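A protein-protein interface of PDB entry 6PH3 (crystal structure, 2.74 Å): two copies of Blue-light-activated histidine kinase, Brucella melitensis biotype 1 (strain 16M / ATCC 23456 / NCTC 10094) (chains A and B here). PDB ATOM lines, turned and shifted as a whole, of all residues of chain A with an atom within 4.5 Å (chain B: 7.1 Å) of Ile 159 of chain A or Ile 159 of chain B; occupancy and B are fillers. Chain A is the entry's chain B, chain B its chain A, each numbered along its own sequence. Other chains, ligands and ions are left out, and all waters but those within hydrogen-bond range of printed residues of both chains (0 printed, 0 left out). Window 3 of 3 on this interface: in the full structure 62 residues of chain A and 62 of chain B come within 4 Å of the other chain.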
ATOM      1  N   ILE A 153      27.213 -16.173  29.551  1.00  0.00           N
ATOM      2  CA  ILE A 153      25.884 -16.783  29.495  1.00  0.00           C
ATOM      3  C   ILE A 153      25.857 -18.075  30.285  1.00  0.00           C
ATOM      4  O   ILE A 153      24.951 -18.271  31.102  1.00  0.00           O
ATOM      5  CB  ILE A 153      25.380 -16.994  28.047  1.00  0.00           C
ATOM      6  CG1 ILE A 153      25.214 -15.666  27.326  1.00  0.00           C
ATOM      7  CG2 ILE A 153      24.042 -17.765  28.041  1.00  0.00           C
ATOM      8  CD1 ILE A 153      25.131 -15.789  25.897  1.00  0.00           C
ATOM      9  N   VAL A 154      26.850 -18.957  30.055  1.00  0.00           N
ATOM     10  CA  VAL A 154      26.884 -20.255  30.727  1.00  0.00           C
ATOM     11  C   VAL A 154      27.034 -20.091  32.269  1.00  0.00           C
ATOM     12  O   VAL A 154      26.443 -20.868  33.016  1.00  0.00           O
ATOM     13  CB  VAL A 154      27.908 -21.244  30.096  1.00  0.00           C
ATOM     14  CG1 VAL A 154      27.898 -22.570  30.804  1.00  0.00           C
ATOM     15  CG2 VAL A 154      27.648 -21.462  28.602  1.00  0.00           C
ATOM     16  N   ALA A 157      23.397 -17.499  33.396  1.00  0.00           N
ATOM     17  CA  ALA A 157      22.180 -18.313  33.202  1.00  0.00           C
ATOM     18  C   ALA A 157      22.647 -19.675  33.669  1.00  0.00           C
ATOM     19  O   ALA A 157      23.814 -19.932  33.374  1.00  0.00           O
ATOM     20  CB  ALA A 157      21.827 -18.350  31.729  1.00  0.00           C
ATOM     21  N   ASN A 158      22.014 -20.438  34.532  1.00  0.00           N
ATOM     22  CA  ASN A 158      22.858 -21.586  34.902  1.00  0.00           C
ATOM     23  C   ASN A 158      22.765 -22.730  33.868  1.00  0.00           C
ATOM     24  O   ASN A 158      21.916 -23.631  33.997  1.00  0.00           O
ATOM     25  CB  ASN A 158      22.642 -22.037  36.345  1.00  0.00           C
ATOM     26  CG  ASN A 158      23.807 -21.638  37.216  1.00  0.00           C
ATOM     27  OD1 ASN A 158      24.978 -21.660  36.791  1.00  0.00           O
ATOM     28  ND2 ASN A 158      23.511 -21.247  38.449  1.00  0.00           N
ATOM     29  N   ILE A 159      23.650 -22.659  32.825  1.00  0.00           N
ATOM     30  CA  ILE A 159      23.560 -23.604  31.720  1.00  0.00           C
ATOM     31  C   ILE A 159      24.545 -24.742  31.863  1.00  0.00           C
ATOM     32  O   ILE A 159      25.742 -24.533  32.075  1.00  0.00           O
ATOM     33  CB  ILE A 159      23.617 -22.946  30.290  1.00  0.00           C
ATOM     34  CG1 ILE A 159      22.762 -21.675  30.154  1.00  0.00           C
ATOM     35  CG2 ILE A 159      23.258 -23.926  29.183  1.00  0.00           C
ATOM     36  CD1 ILE A 159      21.183 -21.803  30.524  1.00  0.00           C
ATOM     37  N   GLY A 160      23.988 -25.947  31.768  1.00  0.00           N
ATOM     38  CA  GLY A 160      24.715 -27.197  31.738  1.00  0.00           C
ATOM     39  C   GLY A 160      25.023 -27.437  30.281  1.00  0.00           C
ATOM     40  O   GLY A 160      24.245 -28.062  29.567  1.00  0.00           O
ATOM     41  N   PHE A 161      26.098 -26.821  29.807  1.00  0.00           N
ATOM     42  CA  PHE A 161      26.514 -26.890  28.415  1.00  0.00           C
ATOM     43  C   PHE A 161      27.817 -27.640  28.279  1.00  0.00           C
ATOM     44  O   PHE A 161      28.747 -27.471  29.076  1.00  0.00           O
ATOM     45  CB  PHE A 161      26.620 -25.472  27.824  1.00  0.00           C
ATOM     46  CG  PHE A 161      27.194 -25.325  26.433  1.00  0.00           C
ATOM     47  CD1 PHE A 161      26.418 -25.602  25.307  1.00  0.00           C
ATOM     48  CD2 PHE A 161      28.479 -24.824  26.244  1.00  0.00           C
ATOM     49  CE1 PHE A 161      26.929 -25.409  24.022  1.00  0.00           C
ATOM     50  CE2 PHE A 161      28.985 -24.623  24.962  1.00  0.00           C
ATOM     51  CZ  PHE A 161      28.211 -24.927  23.859  1.00  0.00           C
ATOM     52  N   SER A 174      30.418 -27.452  31.509  1.00  0.00           N
ATOM     53  CA  SER A 174      30.280 -26.225  32.277  1.00  0.00           C
ATOM     54  C   SER A 174      30.168 -26.632  33.740  1.00  0.00           C
ATOM     55  O   SER A 174      29.907 -27.811  34.037  1.00  0.00           O
ATOM     56  CB  SER A 174      29.064 -25.427  31.832  1.00  0.00           C
ATOM     57  OG  SER A 174      27.880 -26.192  31.872  1.00  0.00           O
ATOM     58  N   GLU A 176      27.841 -26.163  35.789  1.00  0.00           N
ATOM     59  CA  GLU A 176      26.482 -26.690  36.002  1.00  0.00           C
ATOM     60  C   GLU A 176      26.357 -28.116  35.442  1.00  0.00           C
ATOM     61  O   GLU A 176      25.754 -28.978  36.084  1.00  0.00           O
ATOM     62  CB  GLU A 176      25.431 -25.752  35.380  1.00  0.00           C
ATOM     63  CG  GLU A 176      24.008 -26.294  35.345  1.00  0.00           C
ATOM     64  CD  GLU A 176      23.247 -26.508  36.645  1.00  0.00           C
ATOM     65  OE1 GLU A 176      23.843 -26.366  37.739  1.00  0.00           O
ATOM     66  OE2 GLU A 176      22.033 -26.813  36.559  1.00  0.00           O
ATOM     67  N   ILE A 252      23.015 -29.161  25.610  1.00  0.00           N
ATOM     68  CA  ILE A 252      22.524 -28.560  26.842  1.00  0.00           C
ATOM     69  C   ILE A 252      21.779 -29.615  27.675  1.00  0.00           C
ATOM     70  O   ILE A 252      20.705 -30.084  27.289  1.00  0.00           O
ATOM     71  CB  ILE A 252      21.692 -27.269  26.584  1.00  0.00           C
ATOM     72  CG1 ILE A 252      22.540 -26.192  25.831  1.00  0.00           C
ATOM     73  CG2 ILE A 252      21.098 -26.722  27.911  1.00  0.00           C
ATOM     74  CD1 ILE A 252      21.756 -25.051  25.188  1.00  0.00           C
ATOM     75  N   ILE B 153      23.122 -21.787  22.373  1.00  0.00           N
ATOM     76  CA  ILE B 153      22.777 -21.663  23.795  1.00  0.00           C
ATOM     77  C   ILE B 153      21.620 -20.702  23.986  1.00  0.00           C
ATOM     78  O   ILE B 153      20.654 -21.035  24.687  1.00  0.00           O
ATOM     79  CB  ILE B 153      24.008 -21.275  24.678  1.00  0.00           C
ATOM     80  CG1 ILE B 153      25.058 -22.374  24.662  1.00  0.00           C
ATOM     81  CG2 ILE B 153      23.603 -20.938  26.110  1.00  0.00           C
ATOM     82  CD1 ILE B 153      26.365 -21.938  25.094  1.00  0.00           C
ATOM     83  N   VAL B 154      21.709 -19.517  23.350  1.00  0.00           N
ATOM     84  CA  VAL B 154      20.678 -18.493  23.512  1.00  0.00           C
ATOM     85  C   VAL B 154      19.339 -18.956  22.945  1.00  0.00           C
ATOM     86  O   VAL B 154      18.314 -18.640  23.540  1.00  0.00           O
ATOM     87  CB  VAL B 154      21.080 -17.076  23.029  1.00  0.00           C
ATOM     88  CG1 VAL B 154      22.354 -16.599  23.717  1.00  0.00           C
ATOM     89  CG2 VAL B 154      21.186 -16.986  21.511  1.00  0.00           C
ATOM     90  N   GLU B 155      19.339 -19.738  21.861  1.00  0.00           N
ATOM     91  CA  GLU B 155      18.097 -20.231  21.271  1.00  0.00           C
ATOM     92  C   GLU B 155      17.514 -21.424  22.031  1.00  0.00           C
ATOM     93  O   GLU B 155      16.310 -21.438  22.297  1.00  0.00           O
ATOM     94  CB  GLU B 155      18.279 -20.568  19.781  1.00  0.00           C
ATOM     95  CG  GLU B 155      16.959 -20.768  19.060  1.00  0.00           C
ATOM     96  CD  GLU B 155      17.006 -20.912  17.553  1.00  0.00           C
ATOM     97  OE1 GLU B 155      17.754 -20.152  16.893  1.00  0.00           O
ATOM     98  OE2 GLU B 155      16.221 -21.735  17.026  1.00  0.00           O
ATOM     99  N   VAL B 156      18.363 -22.432  22.351  1.00  0.00           N
ATOM    100  CA  VAL B 156      17.957 -23.674  23.019  1.00  0.00           C
ATOM    101  C   VAL B 156      17.586 -23.434  24.487  1.00  0.00           C
ATOM    102  O   VAL B 156      16.497 -23.839  24.897  1.00  0.00           O
ATOM    103  CB  VAL B 156      19.004 -24.802  22.816  1.00  0.00           C
ATOM    104  CG1 VAL B 156      18.661 -26.049  23.636  1.00  0.00           C
ATOM    105  CG2 VAL B 156      19.119 -25.158  21.336  1.00  0.00           C
ATOM    106  N   ALA B 157      18.462 -22.764  25.260  1.00  0.00           N
ATOM    107  CA  ALA B 157      18.199 -22.432  26.662  1.00  0.00           C
ATOM    108  C   ALA B 157      17.239 -21.220  26.787  1.00  0.00           C
ATOM    109  O   ALA B 157      16.845 -20.865  27.909  1.00  0.00           O
ATOM    110  CB  ALA B 157      19.510 -22.160  27.386  1.00  0.00           C
ATOM    111  N   ASN B 158      16.803 -20.653  25.652  1.00  0.00           N
ATOM    112  CA  ASN B 158      15.920 -19.489  25.559  1.00  0.00           C
ATOM    113  C   ASN B 158      16.277 -18.378  26.608  1.00  0.00           C
ATOM    114  O   ASN B 158      15.584 -18.159  27.623  1.00  0.00           O
ATOM    115  CB  ASN B 158      14.450 -19.869  25.557  1.00  0.00           C
ATOM    116  CG  ASN B 158      13.704 -19.018  24.580  1.00  0.00           C
ATOM    117  OD1 ASN B 158      12.786 -18.288  24.955  1.00  0.00           O
ATOM    118  ND2 ASN B 158      14.130 -19.027  23.314  1.00  0.00           N
ATOM    119  N   ILE B 159      17.446 -17.751  26.340  1.00  0.00           N
ATOM    120  CA  ILE B 159      18.071 -16.672  27.095  1.00  0.00           C
ATOM    121  C   ILE B 159      17.820 -15.358  26.374  1.00  0.00           C
ATOM    122  O   ILE B 159      17.992 -15.268  25.154  1.00  0.00           O
ATOM    123  CB  ILE B 159      19.613 -16.907  27.310  1.00  0.00           C
ATOM    124  CG1 ILE B 159      19.959 -18.361  27.832  1.00  0.00           C
ATOM    125  CG2 ILE B 159      20.245 -15.815  28.202  1.00  0.00           C
ATOM    126  CD1 ILE B 159      19.295 -18.834  29.159  1.00  0.00           C
ATOM    127  N   GLY B 160      17.385 -14.366  27.147  1.00  0.00           N
ATOM    128  CA  GLY B 160      17.180 -13.000  26.701  1.00  0.00           C
ATOM    129  C   GLY B 160      18.505 -12.312  26.897  1.00  0.00           C
ATOM    130  O   GLY B 160      18.771 -11.762  27.960  1.00  0.00           O
ATOM    131  N   PHE B 161      19.382 -12.461  25.927  1.00  0.00           N
ATOM    132  CA  PHE B 161      20.731 -11.915  25.963  1.00  0.00           C
ATOM    133  C   PHE B 161      20.908 -10.807  24.932  1.00  0.00           C
ATOM    134  O   PHE B 161      20.460 -10.915  23.779  1.00  0.00           O
ATOM    135  CB  PHE B 161      21.770 -13.043  25.787  1.00  0.00           C
ATOM    136  CG  PHE B 161      23.221 -12.643  25.632  1.00  0.00           C
ATOM    137  CD1 PHE B 161      23.998 -12.324  26.744  1.00  0.00           C
ATOM    138  CD2 PHE B 161      23.835 -12.650  24.380  1.00  0.00           C
ATOM    139  CE1 PHE B 161      25.352 -12.002  26.606  1.00  0.00           C
ATOM    140  CE2 PHE B 161      25.188 -12.322  24.244  1.00  0.00           C
ATOM    141  CZ  PHE B 161      25.934 -11.997  25.355  1.00  0.00           C
ATOM    142  N   TRP B 162      21.541  -9.728  25.379  1.00  0.00           N
ATOM    143  CA  TRP B 162      21.847  -8.585  24.545  1.00  0.00           C
ATOM    144  C   TRP B 162      23.270  -8.158  24.755  1.00  0.00           C
ATOM    145  O   TRP B 162      23.876  -8.431  25.801  1.00  0.00           O
ATOM    146  CB  TRP B 162      20.880  -7.398  24.792  1.00  0.00           C
ATOM    147  CG  TRP B 162      20.770  -6.916  26.216  1.00  0.00           C
ATOM    148  CD1 TRP B 162      19.736  -7.144  27.079  1.00  0.00           C
ATOM    149  CD2 TRP B 162      21.701  -6.071  26.920  1.00  0.00           C
ATOM    150  NE1 TRP B 162      19.975  -6.519  28.286  1.00  0.00           N
ATOM    151  CE2 TRP B 162      21.180  -5.865  28.220  1.00  0.00           C
ATOM    152  CE3 TRP B 162      22.944  -5.496  26.591  1.00  0.00           C
ATOM    153  CZ2 TRP B 162      21.869  -5.120  29.197  1.00  0.00           C
ATOM    154  CZ3 TRP B 162      23.629  -4.772  27.560  1.00  0.00           C
ATOM    155  CH2 TRP B 162      23.092  -4.580  28.840  1.00  0.00           C
ATOM    156  N   CYS B 173      20.154  -8.408  19.961  1.00  0.00           N
ATOM    157  CA  CYS B 173      19.120  -8.903  20.870  1.00  0.00           C
ATOM    158  C   CYS B 173      18.718 -10.290  20.490  1.00  0.00           C
ATOM    159  O   CYS B 173      18.294 -10.484  19.350  1.00  0.00           O
ATOM    160  CB  CYS B 173      17.903  -7.978  20.835  1.00  0.00           C
ATOM    161  SG  CYS B 173      18.133  -6.369  21.636  1.00  0.00           S
ATOM    162  N   SER B 174      18.724 -11.237  21.454  1.00  0.00           N
ATOM    163  CA  SER B 174      18.294 -12.607  21.155  1.00  0.00           C
ATOM    164  C   SER B 174      16.799 -12.638  20.897  1.00  0.00           C
ATOM    165  O   SER B 174      16.102 -11.692  21.243  1.00  0.00           O
ATOM    166  CB  SER B 174      18.664 -13.552  22.283  1.00  0.00           C
ATOM    167  OG  SER B 174      18.096 -13.110  23.499  1.00  0.00           O
ATOM    168  N   ALA B 175      16.307 -13.691  20.244  1.00  0.00           N
ATOM    169  CA  ALA B 175      14.878 -13.876  19.944  1.00  0.00           C
ATOM    170  C   ALA B 175      13.997 -13.715  21.200  1.00  0.00           C
ATOM    171  O   ALA B 175      12.882 -13.199  21.095  1.00  0.00           O
ATOM    172  CB  ALA B 175      14.655 -15.256  19.327  1.00  0.00           C
ATOM    173  N   GLU B 176      14.511 -14.159  22.377  1.00  0.00           N
ATOM    174  CA  GLU B 176      13.842 -14.075  23.682  1.00  0.00           C
ATOM    175  C   GLU B 176      13.872 -12.633  24.224  1.00  0.00           C
ATOM    176  O   GLU B 176      12.875 -12.150  24.756  1.00  0.00           O
ATOM    177  CB  GLU B 176      14.471 -15.061  24.675  1.00  0.00           C
ATOM    178  CG  GLU B 176      13.993 -14.935  26.107  1.00  0.00           C
ATOM    179  CD  GLU B 176      12.556 -15.310  26.429  1.00  0.00           C
ATOM    180  OE1 GLU B 176      11.755 -15.561  25.497  1.00  0.00           O
ATOM    181  OE2 GLU B 176      12.230 -15.342  27.640  1.00  0.00           O
ATOM    182  N   CYS B 177      15.019 -11.954  24.073  1.00  0.00           N
ATOM    183  CA  CYS B 177      15.223 -10.573  24.480  1.00  0.00           C
ATOM    184  C   CYS B 177      14.207  -9.696  23.732  1.00  0.00           C
ATOM    185  O   CYS B 177      13.526  -8.885  24.372  1.00  0.00           O
ATOM    186  CB  CYS B 177      16.662 -10.159  24.188  1.00  0.00           C
ATOM    187  SG  CYS B 177      17.031  -8.441  24.584  1.00  0.00           S
ATOM    188  N   ILE B 180      10.594 -10.244  24.994  1.00  0.00           N
ATOM    189  CA  ILE B 180      10.447  -9.653  26.324  1.00  0.00           C
ATOM    190  C   ILE B 180       9.986  -8.190  26.155  1.00  0.00           C
ATOM    191  O   ILE B 180       8.990  -7.801  26.761  1.00  0.00           O
ATOM    192  CB  ILE B 180      11.706  -9.863  27.229  1.00  0.00           C
ATOM    193  CG1 ILE B 180      11.808 -11.323  27.703  1.00  0.00           C
ATOM    194  CG2 ILE B 180      11.682  -8.926  28.439  1.00  0.00           C
ATOM    195  CD1 ILE B 180      13.218 -11.765  28.142  1.00  0.00           C
ATOM    196  N   GLY B 251      24.481  -8.391  28.764  1.00  0.00           N
ATOM    197  CA  GLY B 251      23.407  -8.502  29.736  1.00  0.00           C
ATOM    198  C   GLY B 251      22.384  -9.563  29.423  1.00  0.00           C
ATOM    199  O   GLY B 251      22.095  -9.839  28.254  1.00  0.00           O
ATOM    200  N   ILE B 252      21.837 -10.168  30.482  1.00  0.00           N
ATOM    201  CA  ILE B 252      20.738 -11.131  30.400  1.00  0.00           C
ATOM    202  C   ILE B 252      19.522 -10.486  31.079  1.00  0.00           C
ATOM    203  O   ILE B 252      19.608 -10.050  32.228  1.00  0.00           O
ATOM    204  CB  ILE B 252      21.064 -12.549  30.938  1.00  0.00           C
ATOM    205  CG1 ILE B 252      22.073 -13.293  30.036  1.00  0.00           C
ATOM    206  CG2 ILE B 252      19.794 -13.352  31.120  1.00  0.00           C
ATOM    207  CD1 ILE B 252      23.096 -14.108  30.749  1.00  0.00           C
ATOM    208  N   VAL B 253      18.428 -10.358  30.314  1.00  0.00           N
ATOM    209  CA  VAL B 253      17.135  -9.811  30.737  1.00  0.00           C
ATOM    210  C   VAL B 253      16.123 -10.930  30.986  1.00  0.00           C
ATOM    211  O   VAL B 253      16.060 -11.904  30.244  1.00  0.00           O
ATOM    212  CB  VAL B 253      16.599  -8.703  29.758  1.00  0.00           C
ATOM    213  CG1 VAL B 253      16.325  -9.244  28.348  1.00  0.00           C
ATOM    214  CG2 VAL B 253      15.395  -7.944  30.327  1.00  0.00           C
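O of Val 154 of chain B is in hydrogen-bond range of N of Ile 159 of chain B, at 3.1 Å. OG of Ser 174 of chain B is in hydrogen-bond range of O of Ile 159 of chain B (2.7 Å). The backbone NH (N) of Phe 161 of chain B lies within hydrogen-bond range of the side-chain hydroxyl (OG) of Ser 174 of chain B. The backbone NH (N) of Ile 159 of chain A lies within hydrogen-bond range of the backbone carbonyl oxygen (O) of Val 154 of chain A (3.3 Å). OG of Ser 174 of chain A lies within hydrogen-bond range of O of Ile 159 of chain A, at 2.7 Å. OG of Ser 174 of chain A lies within hydrogen-bond range of N of Phe 161 of chain A, 2.8 Å away.
Of the 19 printed residues of chain B, 6 touch a printed residue of chain A. Printed residues of chain B that touch a printed residue of chain A: Ile 153, Val 154, Val 156, Ala 157, Ile 159 and Phe 161. Of the 10 printed residues of chain A, 6 touch a printed residue of chain B. Along chain A the printed residues that touch a printed residue of chain B span positions 153 to 252. Among the printed residues, 10 pairs touch across the chains.
Ile 153 of chain A touches Ile 153 of chain B (CG2 to CG2, 3.7 Å). Val 154 of chain B touches Ile 153 of chain A. CD1 of Phe 161 of chain B touches CG1 of Ile 153 of chain A (3.6 Å). CD1 of Ile 153 of chain B touches CG2 of Val 154 of chain A, 3.8 Å away. Ala 157 of chain A touches Ile 159 of chain B (CB to CD1, 3.6 Å). Ala 157 of chain B touches Ile 159 of chain A (CB to CD1, 3.6 Å). Ile 159 of chain A touches Ile 159 of chain B (CD1 to CD1, 3.8 Å). CD1 of Phe 161 of chain A touches CG1 of Ile 153 of chain B (3.6 Å). CD1 of Ile 252 of chain A touches CA of Ile 153 of chain B, 3.8 Å away. Ile 252 of chain A touches Val 156 of chain B.
Of the printed residues of chain B, Ile 153 of chain A touches Ile 153, Val 154 and Phe 161. Of the printed residues of chain B, Ala 157 of chain A touches Ile 159 (3.6 Å). Ile 159 of chain A touches just these residues of chain B: Ala 157 (3.6 Å) and Ile 159 (3.8 Å). Glu 155 of chain B touches none of the printed residues of chain A. Of chain A, only Ala 157 and Ile 159 come within 4 Å of Ile 159 of chain B. Printed residues of chain A within 4 Å of Phe 161 of chain B: Ile 153 (3.6 Å). The nearest residue of chain B that does not touch Ile 159 of chain A is Ile 153 of chain B (4.2 Å). The nearest residue of chain A that does not touch Ile 159 of chain B is Ile 153 of chain A (4.1 Å). The nearest printed residue of chain A that does not touch Ala 157 of chain B is Ile 252 of chain A (4.01 Å).
Ile 153 of chain B touches its own counterpart, Ile 153 of chain A. Ile 153 of chain A touches Phe 161 of chain B, and with the chains exchanged Phe 161 of chain A touches Ile 153 of chain B. Ile 159 of chain A touches its own counterpart, Ile 159 of chain B. Ile 252 of chain A touches Ile 153 of chain B, but with the chains exchanged Ile 153 of chain A does not touch Ile 252 of chain B (4.1 Å). Positions printed for both chains: 153, 154, 157, 158, 159, 160, 161, 174, 176 and 252.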
